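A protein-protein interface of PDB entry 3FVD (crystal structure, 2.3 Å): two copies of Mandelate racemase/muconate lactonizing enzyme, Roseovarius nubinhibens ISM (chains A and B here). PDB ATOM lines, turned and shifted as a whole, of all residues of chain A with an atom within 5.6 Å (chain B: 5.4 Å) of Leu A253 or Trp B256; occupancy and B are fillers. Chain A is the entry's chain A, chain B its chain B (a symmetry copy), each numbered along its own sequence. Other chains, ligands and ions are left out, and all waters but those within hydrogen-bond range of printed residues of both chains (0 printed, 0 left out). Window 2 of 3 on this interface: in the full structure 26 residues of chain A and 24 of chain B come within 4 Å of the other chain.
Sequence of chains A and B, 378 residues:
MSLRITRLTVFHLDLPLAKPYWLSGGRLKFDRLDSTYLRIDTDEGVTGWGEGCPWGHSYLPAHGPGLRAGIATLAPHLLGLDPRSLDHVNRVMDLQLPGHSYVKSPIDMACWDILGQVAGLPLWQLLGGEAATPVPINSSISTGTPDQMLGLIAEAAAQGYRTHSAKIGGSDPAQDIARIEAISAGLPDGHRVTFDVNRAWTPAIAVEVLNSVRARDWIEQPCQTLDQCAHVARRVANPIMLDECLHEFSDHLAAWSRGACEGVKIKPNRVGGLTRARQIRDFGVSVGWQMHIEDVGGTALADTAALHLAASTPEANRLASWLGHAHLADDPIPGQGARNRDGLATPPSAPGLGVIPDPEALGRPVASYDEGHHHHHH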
ATOM      1  N   PHE A 249       2.739  -2.776  30.262  1.00  0.00           N
ATOM      2  CA  PHE A 249       2.249  -3.443  29.087  1.00  0.00           C
ATOM      3  C   PHE A 249       3.201  -3.295  27.870  1.00  0.00           C
ATOM      4  O   PHE A 249       3.376  -4.240  27.073  1.00  0.00           O
ATOM      5  CB  PHE A 249       0.836  -2.918  28.786  1.00  0.00           C
ATOM      6  CG  PHE A 249       0.219  -3.576  27.593  1.00  0.00           C
ATOM      7  CD1 PHE A 249      -0.339  -4.836  27.712  1.00  0.00           C
ATOM      8  CD2 PHE A 249       0.263  -2.969  26.319  1.00  0.00           C
ATOM      9  CE1 PHE A 249      -0.883  -5.494  26.610  1.00  0.00           C
ATOM     10  CE2 PHE A 249      -0.322  -3.587  25.231  1.00  0.00           C
ATOM     11  CZ  PHE A 249      -0.913  -4.873  25.390  1.00  0.00           C
ATOM     12  N   SER A 250       3.832  -2.117  27.714  1.00  0.00           N
ATOM     13  CA  SER A 250       4.703  -1.868  26.538  1.00  0.00           C
ATOM     14  C   SER A 250       5.936  -2.752  26.510  1.00  0.00           C
ATOM     15  O   SER A 250       6.490  -2.990  25.438  1.00  0.00           O
ATOM     16  CB  SER A 250       5.164  -0.370  26.471  1.00  0.00           C
ATOM     17  OG  SER A 250       5.938  -0.005  27.616  1.00  0.00           O
ATOM     18  N   ASP A 251       6.398  -3.191  27.691  1.00  0.00           N
ATOM     19  CA  ASP A 251       7.523  -4.146  27.774  1.00  0.00           C
ATOM     20  C   ASP A 251       7.092  -5.495  27.260  1.00  0.00           C
ATOM     21  O   ASP A 251       7.885  -6.155  26.601  1.00  0.00           O
ATOM     22  CB  ASP A 251       7.961  -4.303  29.200  1.00  0.00           C
ATOM     23  CG  ASP A 251       8.549  -3.031  29.752  1.00  0.00           C
ATOM     24  OD1 ASP A 251       8.230  -2.699  30.874  1.00  0.00           O
ATOM     25  OD2 ASP A 251       9.353  -2.351  29.057  1.00  0.00           O
ATOM     26  N   HIS A 252       5.819  -5.865  27.476  1.00  0.00           N
ATOM     27  CA  HIS A 252       5.263  -7.146  26.989  1.00  0.00           C
ATOM     28  C   HIS A 252       5.108  -7.091  25.474  1.00  0.00           C
ATOM     29  O   HIS A 252       5.482  -8.022  24.736  1.00  0.00           O
ATOM     30  CB  HIS A 252       3.940  -7.448  27.677  1.00  0.00           C
ATOM     31  CG  HIS A 252       4.073  -7.617  29.166  1.00  0.00           C
ATOM     32  ND1 HIS A 252       4.234  -6.552  30.049  1.00  0.00           N
ATOM     33  CD2 HIS A 252       4.034  -8.738  29.939  1.00  0.00           C
ATOM     34  CE1 HIS A 252       4.296  -7.016  31.293  1.00  0.00           C
ATOM     35  NE2 HIS A 252       4.175  -8.336  31.253  1.00  0.00           N
ATOM     36  N   LEU A 253       4.604  -5.972  24.984  1.00  0.00           N
ATOM     37  CA  LEU A 253       4.531  -5.768  23.520  1.00  0.00           C
ATOM     38  C   LEU A 253       5.894  -5.853  22.864  1.00  0.00           C
ATOM     39  O   LEU A 253       6.052  -6.514  21.821  1.00  0.00           O
ATOM     40  CB  LEU A 253       4.006  -4.353  23.265  1.00  0.00           C
ATOM     41  CG  LEU A 253       2.957  -4.039  22.251  1.00  0.00           C
ATOM     42  CD1 LEU A 253       1.978  -5.198  22.210  1.00  0.00           C
ATOM     43  CD2 LEU A 253       2.289  -2.712  22.746  1.00  0.00           C
ATOM     44  N   ALA A 254       6.905  -5.182  23.456  1.00  0.00           N
ATOM     45  CA  ALA A 254       8.293  -5.278  22.943  1.00  0.00           C
ATOM     46  C   ALA A 254       8.800  -6.741  22.996  1.00  0.00           C
ATOM     47  O   ALA A 254       9.436  -7.218  22.072  1.00  0.00           O
ATOM     48  CB  ALA A 254       9.217  -4.370  23.845  1.00  0.00           C
ATOM     49  N   ALA A 255       8.487  -7.472  24.073  1.00  0.00           N
ATOM     50  CA  ALA A 255       8.943  -8.860  24.239  1.00  0.00           C
ATOM     51  C   ALA A 255       8.306  -9.634  23.109  1.00  0.00           C
ATOM     52  O   ALA A 255       8.948 -10.384  22.404  1.00  0.00           O
ATOM     53  CB  ALA A 255       8.483  -9.405  25.564  1.00  0.00           C
ATOM     54  N   TRP A 256       7.037  -9.391  22.874  1.00  0.00           N
ATOM     55  CA  TRP A 256       6.356 -10.143  21.811  1.00  0.00           C
ATOM     56  C   TRP A 256       6.970  -9.791  20.451  1.00  0.00           C
ATOM     57  O   TRP A 256       7.247 -10.668  19.615  1.00  0.00           O
ATOM     58  CB  TRP A 256       4.865  -9.830  21.835  1.00  0.00           C
ATOM     59  CG  TRP A 256       4.199 -10.346  20.598  1.00  0.00           C
ATOM     60  CD1 TRP A 256       3.800 -11.645  20.342  1.00  0.00           C
ATOM     61  CD2 TRP A 256       3.901  -9.592  19.438  1.00  0.00           C
ATOM     62  NE1 TRP A 256       3.295 -11.727  19.067  1.00  0.00           N
ATOM     63  CE2 TRP A 256       3.356 -10.488  18.486  1.00  0.00           C
ATOM     64  CE3 TRP A 256       4.095  -8.242  19.085  1.00  0.00           C
ATOM     65  CZ2 TRP A 256       2.954 -10.077  17.198  1.00  0.00           C
ATOM     66  CZ3 TRP A 256       3.709  -7.814  17.789  1.00  0.00           C
ATOM     67  CH2 TRP A 256       3.142  -8.738  16.869  1.00  0.00           C
ATOM     68  N   SER A 257       7.192  -8.501  20.205  1.00  0.00           N
ATOM     69  CA  SER A 257       7.623  -8.114  18.878  1.00  0.00           C
ATOM     70  C   SER A 257       9.070  -8.539  18.559  1.00  0.00           C
ATOM     71  O   SER A 257       9.368  -8.751  17.393  1.00  0.00           O
ATOM     72  CB  SER A 257       7.386  -6.589  18.644  1.00  0.00           C
ATOM     73  OG  SER A 257       8.558  -5.836  18.690  1.00  0.00           O
ATOM     74  N   ARG A 258       9.936  -8.597  19.595  1.00  0.00           N
ATOM     75  CA  ARG A 258      11.295  -9.097  19.473  1.00  0.00           C
ATOM     76  C   ARG A 258      11.328 -10.644  19.382  1.00  0.00           C
ATOM     77  O   ARG A 258      12.390 -11.252  19.160  1.00  0.00           O
ATOM     78  CB  ARG A 258      12.130  -8.646  20.689  1.00  0.00           C
ATOM     79  CG  ARG A 258      12.751  -7.236  20.617  1.00  0.00           C
ATOM     80  CD  ARG A 258      13.148  -6.777  22.019  1.00  0.00           C
ATOM     81  NE  ARG A 258      14.408  -6.016  22.123  1.00  0.00           N
ATOM     82  CZ  ARG A 258      15.548  -6.370  21.537  1.00  0.00           C
ATOM     83  NH1 ARG A 258      15.624  -7.433  20.721  1.00  0.00           N
ATOM     84  NH2 ARG A 258      16.629  -5.637  21.743  1.00  0.00           N
ATOM     85  N   PHE A 283      -3.552 -10.572  26.624  1.00  0.00           N
ATOM     86  CA  PHE A 283      -2.645 -10.405  25.531  1.00  0.00           C
ATOM     87  C   PHE A 283      -1.866 -11.735  25.402  1.00  0.00           C
ATOM     88  O   PHE A 283      -1.693 -12.266  24.287  1.00  0.00           O
ATOM     89  CB  PHE A 283      -1.680  -9.209  25.788  1.00  0.00           C
ATOM     90  CG  PHE A 283      -0.611  -9.048  24.687  1.00  0.00           C
ATOM     91  CD1 PHE A 283       0.678  -9.522  24.904  1.00  0.00           C
ATOM     92  CD2 PHE A 283      -0.915  -8.467  23.479  1.00  0.00           C
ATOM     93  CE1 PHE A 283       1.638  -9.449  23.968  1.00  0.00           C
ATOM     94  CE2 PHE A 283       0.055  -8.322  22.512  1.00  0.00           C
ATOM     95  CZ  PHE A 283       1.360  -8.800  22.756  1.00  0.00           C
ATOM     96  N   TRP A 289       1.194 -17.301  24.590  1.00  0.00           N
ATOM     97  CA  TRP A 289       2.120 -17.432  25.686  1.00  0.00           C
ATOM     98  C   TRP A 289       1.537 -18.435  26.730  1.00  0.00           C
ATOM     99  O   TRP A 289       0.302 -18.628  26.854  1.00  0.00           O
ATOM    100  CB  TRP A 289       2.317 -16.087  26.405  1.00  0.00           C
ATOM    101  CG  TRP A 289       3.221 -15.127  25.678  1.00  0.00           C
ATOM    102  CD1 TRP A 289       4.074 -15.411  24.670  1.00  0.00           C
ATOM    103  CD2 TRP A 289       3.448 -13.775  26.015  1.00  0.00           C
ATOM    104  NE1 TRP A 289       4.776 -14.332  24.304  1.00  0.00           N
ATOM    105  CE2 TRP A 289       4.386 -13.290  25.116  1.00  0.00           C
ATOM    106  CE3 TRP A 289       2.865 -12.895  26.950  1.00  0.00           C
ATOM    107  CZ2 TRP A 289       4.840 -11.968  25.153  1.00  0.00           C
ATOM    108  CZ3 TRP A 289       3.293 -11.579  26.988  1.00  0.00           C
ATOM    109  CH2 TRP A 289       4.298 -11.137  26.083  1.00  0.00           C
ATOM    110  N   ASP B 251      -4.791  -8.842  13.752  1.00  0.00           N
ATOM    111  CA  ASP B 251      -4.663  -7.838  12.693  1.00  0.00           C
ATOM    112  C   ASP B 251      -4.339  -6.497  13.311  1.00  0.00           C
ATOM    113  O   ASP B 251      -3.582  -5.739  12.726  1.00  0.00           O
ATOM    114  CB  ASP B 251      -5.942  -7.709  11.870  1.00  0.00           C
ATOM    115  CG  ASP B 251      -6.344  -9.031  11.149  1.00  0.00           C
ATOM    116  OD1 ASP B 251      -7.554  -9.343  11.134  1.00  0.00           O
ATOM    117  OD2 ASP B 251      -5.504  -9.742  10.563  1.00  0.00           O
ATOM    118  N   HIS B 252      -4.833  -6.230  14.519  1.00  0.00           N
ATOM    119  CA  HIS B 252      -4.506  -4.960  15.191  1.00  0.00           C
ATOM    120  C   HIS B 252      -3.040  -4.932  15.590  1.00  0.00           C
ATOM    121  O   HIS B 252      -2.304  -3.954  15.374  1.00  0.00           O
ATOM    122  CB  HIS B 252      -5.415  -4.779  16.393  1.00  0.00           C
ATOM    123  CG  HIS B 252      -6.836  -4.595  16.013  1.00  0.00           C
ATOM    124  ND1 HIS B 252      -7.632  -5.642  15.570  1.00  0.00           N
ATOM    125  CD2 HIS B 252      -7.623  -3.490  15.999  1.00  0.00           C
ATOM    126  CE1 HIS B 252      -8.845  -5.184  15.292  1.00  0.00           C
ATOM    127  NE2 HIS B 252      -8.866  -3.885  15.524  1.00  0.00           N
ATOM    128  N   LEU B 253      -2.607  -6.057  16.110  1.00  0.00           N
ATOM    129  CA  LEU B 253      -1.208  -6.252  16.478  1.00  0.00           C
ATOM    130  C   LEU B 253      -0.292  -6.112  15.287  1.00  0.00           C
ATOM    131  O   LEU B 253       0.730  -5.463  15.351  1.00  0.00           O
ATOM    132  CB  LEU B 253      -1.071  -7.681  17.141  1.00  0.00           C
ATOM    133  CG  LEU B 253      -0.043  -7.906  18.212  1.00  0.00           C
ATOM    134  CD1 LEU B 253      -0.397  -6.913  19.253  1.00  0.00           C
ATOM    135  CD2 LEU B 253      -0.061  -9.370  18.774  1.00  0.00           C
ATOM    136  N   ALA B 254      -0.690  -6.696  14.166  1.00  0.00           N
ATOM    137  CA  ALA B 254       0.017  -6.533  12.896  1.00  0.00           C
ATOM    138  C   ALA B 254      -0.069  -5.028  12.476  1.00  0.00           C
ATOM    139  O   ALA B 254       0.932  -4.404  12.109  1.00  0.00           O
ATOM    140  CB  ALA B 254      -0.680  -7.410  11.858  1.00  0.00           C
ATOM    141  N   ALA B 255      -1.241  -4.406  12.554  1.00  0.00           N
ATOM    142  CA  ALA B 255      -1.272  -2.986  12.140  1.00  0.00           C
ATOM    143  C   ALA B 255      -0.234  -2.179  12.964  1.00  0.00           C
ATOM    144  O   ALA B 255       0.551  -1.381  12.447  1.00  0.00           O
ATOM    145  CB  ALA B 255      -2.704  -2.418  12.342  1.00  0.00           C
ATOM    146  N   TRP B 256      -0.249  -2.401  14.268  1.00  0.00           N
ATOM    147  CA  TRP B 256       0.659  -1.722  15.168  1.00  0.00           C
ATOM    148  C   TRP B 256       2.161  -1.961  14.840  1.00  0.00           C
ATOM    149  O   TRP B 256       2.991  -1.013  14.758  1.00  0.00           O
ATOM    150  CB  TRP B 256       0.382  -2.121  16.614  1.00  0.00           C
ATOM    151  CG  TRP B 256       1.447  -1.554  17.487  1.00  0.00           C
ATOM    152  CD1 TRP B 256       1.538  -0.258  17.918  1.00  0.00           C
ATOM    153  CD2 TRP B 256       2.550  -2.244  18.071  1.00  0.00           C
ATOM    154  NE1 TRP B 256       2.630  -0.097  18.741  1.00  0.00           N
ATOM    155  CE2 TRP B 256       3.298  -1.287  18.819  1.00  0.00           C
ATOM    156  CE3 TRP B 256       3.018  -3.566  17.995  1.00  0.00           C
ATOM    157  CZ2 TRP B 256       4.499  -1.615  19.495  1.00  0.00           C
ATOM    158  CZ3 TRP B 256       4.184  -3.890  18.609  1.00  0.00           C
ATOM    159  CH2 TRP B 256       4.940  -2.910  19.361  1.00  0.00           C
ATOM    160  N   SER B 257       2.517  -3.215  14.598  1.00  0.00           N
ATOM    161  CA  SER B 257       3.934  -3.488  14.424  1.00  0.00           C
ATOM    162  C   SER B 257       4.417  -2.995  13.080  1.00  0.00           C
ATOM    163  O   SER B 257       5.567  -2.741  12.928  1.00  0.00           O
ATOM    164  CB  SER B 257       4.283  -4.981  14.595  1.00  0.00           C
ATOM    165  OG  SER B 257       3.612  -5.746  13.630  1.00  0.00           O
ATOM    166  N   ARG B 258       3.560  -2.877  12.080  1.00  0.00           N
ATOM    167  CA  ARG B 258       4.054  -2.277  10.828  1.00  0.00           C
ATOM    168  C   ARG B 258       4.003  -0.748  10.855  1.00  0.00           C
ATOM    169  O   ARG B 258       4.284  -0.127   9.865  1.00  0.00           O
ATOM    170  CB  ARG B 258       3.254  -2.770   9.630  1.00  0.00           C
ATOM    171  CG  ARG B 258       3.424  -4.256   9.263  1.00  0.00           C
ATOM    172  CD  ARG B 258       2.063  -4.655   8.826  1.00  0.00           C
ATOM    173  NE  ARG B 258       1.874  -5.795   7.919  1.00  0.00           N
ATOM    174  CZ  ARG B 258       2.124  -5.816   6.599  1.00  0.00           C
ATOM    175  NH1 ARG B 258       1.807  -6.925   5.944  1.00  0.00           N
ATOM    176  NH2 ARG B 258       2.730  -4.799   5.941  1.00  0.00           N
ATOM    177  N   GLY B 259       3.631  -0.118  11.955  1.00  0.00           N
ATOM    178  CA  GLY B 259       3.302   1.311  11.891  1.00  0.00           C
ATOM    179  C   GLY B 259       2.309   1.747  10.798  1.00  0.00           C
ATOM    180  O   GLY B 259       2.474   2.803  10.240  1.00  0.00           O
ATOM    181  N   ALA B 260       1.248   0.987  10.548  1.00  0.00           N
ATOM    182  CA  ALA B 260       0.356   1.237   9.448  1.00  0.00           C
ATOM    183  C   ALA B 260      -0.680   2.362   9.693  1.00  0.00           C
ATOM    184  O   ALA B 260      -1.393   2.771   8.746  1.00  0.00           O
ATOM    185  CB  ALA B 260      -0.427  -0.054   9.107  1.00  0.00           C
ATOM    186  N   PHE B 283      -6.030  -2.050  24.018  1.00  0.00           N
ATOM    187  CA  PHE B 283      -4.769  -2.078  23.306  1.00  0.00           C
ATOM    188  C   PHE B 283      -4.557  -0.683  22.674  1.00  0.00           C
ATOM    189  O   PHE B 283      -3.474  -0.151  22.729  1.00  0.00           O
ATOM    190  CB  PHE B 283      -4.778  -3.178  22.220  1.00  0.00           C
ATOM    191  CG  PHE B 283      -3.516  -3.229  21.416  1.00  0.00           C
ATOM    192  CD1 PHE B 283      -3.479  -2.667  20.184  1.00  0.00           C
ATOM    193  CD2 PHE B 283      -2.353  -3.785  21.931  1.00  0.00           C
ATOM    194  CE1 PHE B 283      -2.373  -2.725  19.380  1.00  0.00           C
ATOM    195  CE2 PHE B 283      -1.191  -3.822  21.149  1.00  0.00           C
ATOM    196  CZ  PHE B 283      -1.195  -3.329  19.882  1.00  0.00           C
ATOM    197  N   VAL B 287      -1.214   2.003  23.094  1.00  0.00           N
ATOM    198  CA  VAL B 287      -0.270   2.420  22.000  1.00  0.00           C
ATOM    199  C   VAL B 287      -0.563   3.836  21.454  1.00  0.00           C
ATOM    200  O   VAL B 287       0.073   4.265  20.485  1.00  0.00           O
ATOM    201  CB  VAL B 287      -0.228   1.353  20.847  1.00  0.00           C
ATOM    202  CG1 VAL B 287       0.039  -0.142  21.436  1.00  0.00           C
ATOM    203  CG2 VAL B 287      -1.567   1.242  20.146  1.00  0.00           C
ATOM    204  N   TRP B 289      -3.506   5.138  20.021  1.00  0.00           N
ATOM    205  CA  TRP B 289      -4.385   5.220  18.888  1.00  0.00           C
ATOM    206  C   TRP B 289      -5.590   6.125  19.224  1.00  0.00           C
ATOM    207  O   TRP B 289      -6.028   6.201  20.363  1.00  0.00           O
ATOM    208  CB  TRP B 289      -4.975   3.829  18.588  1.00  0.00           C
ATOM    209  CG  TRP B 289      -4.071   2.987  17.754  1.00  0.00           C
ATOM    210  CD1 TRP B 289      -2.905   3.387  17.175  1.00  0.00           C
ATOM    211  CD2 TRP B 289      -4.249   1.604  17.402  1.00  0.00           C
ATOM    212  NE1 TRP B 289      -2.360   2.364  16.457  1.00  0.00           N
ATOM    213  CE2 TRP B 289      -3.164   1.249  16.584  1.00  0.00           C
ATOM    214  CE3 TRP B 289      -5.220   0.638  17.711  1.00  0.00           C
ATOM    215  CZ2 TRP B 289      -2.979  -0.066  16.087  1.00  0.00           C
ATOM    216  CZ3 TRP B 289      -5.083  -0.638  17.170  1.00  0.00           C
ATOM    217  CH2 TRP B 289      -3.960  -0.980  16.359  1.00  0.00           C
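The backbone carbonyl oxygen of Leu B253 is in hydrogen-bond range of the side-chain hydroxyl of Ser B257.
Among the printed residues, pairs that only touch across the chains: Trp A256 with Leu B253, Phe A283 with Leu B253, Leu A253 with Phe B283, Leu A253 with Val B287, Leu A253 with Trp B256 and Phe A249 with Phe B283.
Leu A253 touches three residues of chain B. Printed residues of chain B within 4 Å of Phe A283: Leu B253. Printed residues of chain B within 4 Å of Trp A256: Leu B253. Of the printed residues of chain A, Val B287 touches Leu A253. Of the printed residues of chain B, Phe A249 touches Phe B283. Printed residues of chain A within 4 Å of Phe B283: Phe A249 (3.9 Å) and Leu A253 (3.6 Å). Trp B289 touches none of the printed residues of chain A. The nearest residue of chain B that does not touch Leu A253 is Leu B253 (4.2 Å). The nearest printed residue of chain A that does not touch Phe B283 is Phe A283 (4.9 Å).
Hydrophobic or aromatic side chains of chain A within 4 Å of the printed part of chain B: Phe A249, Leu A253, Trp A256 and Phe A283. Among the printed residues, 6 pairs touch across the chains. Among the printed residues, no Asp or Glu carboxylate lies within 4 Å of a Lys or Arg side-chain nitrogen of the other chain.
Leu A253 touches Trp B256, and with the chains exchanged Trp A256 touches Leu B253. Leu A253 touches Phe B283, and with the chains exchanged Phe A283 touches Leu B253. Of the 6 pairs that touch across the chains among the printed residues, 4 have their exchanged pair printed and touching as well.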
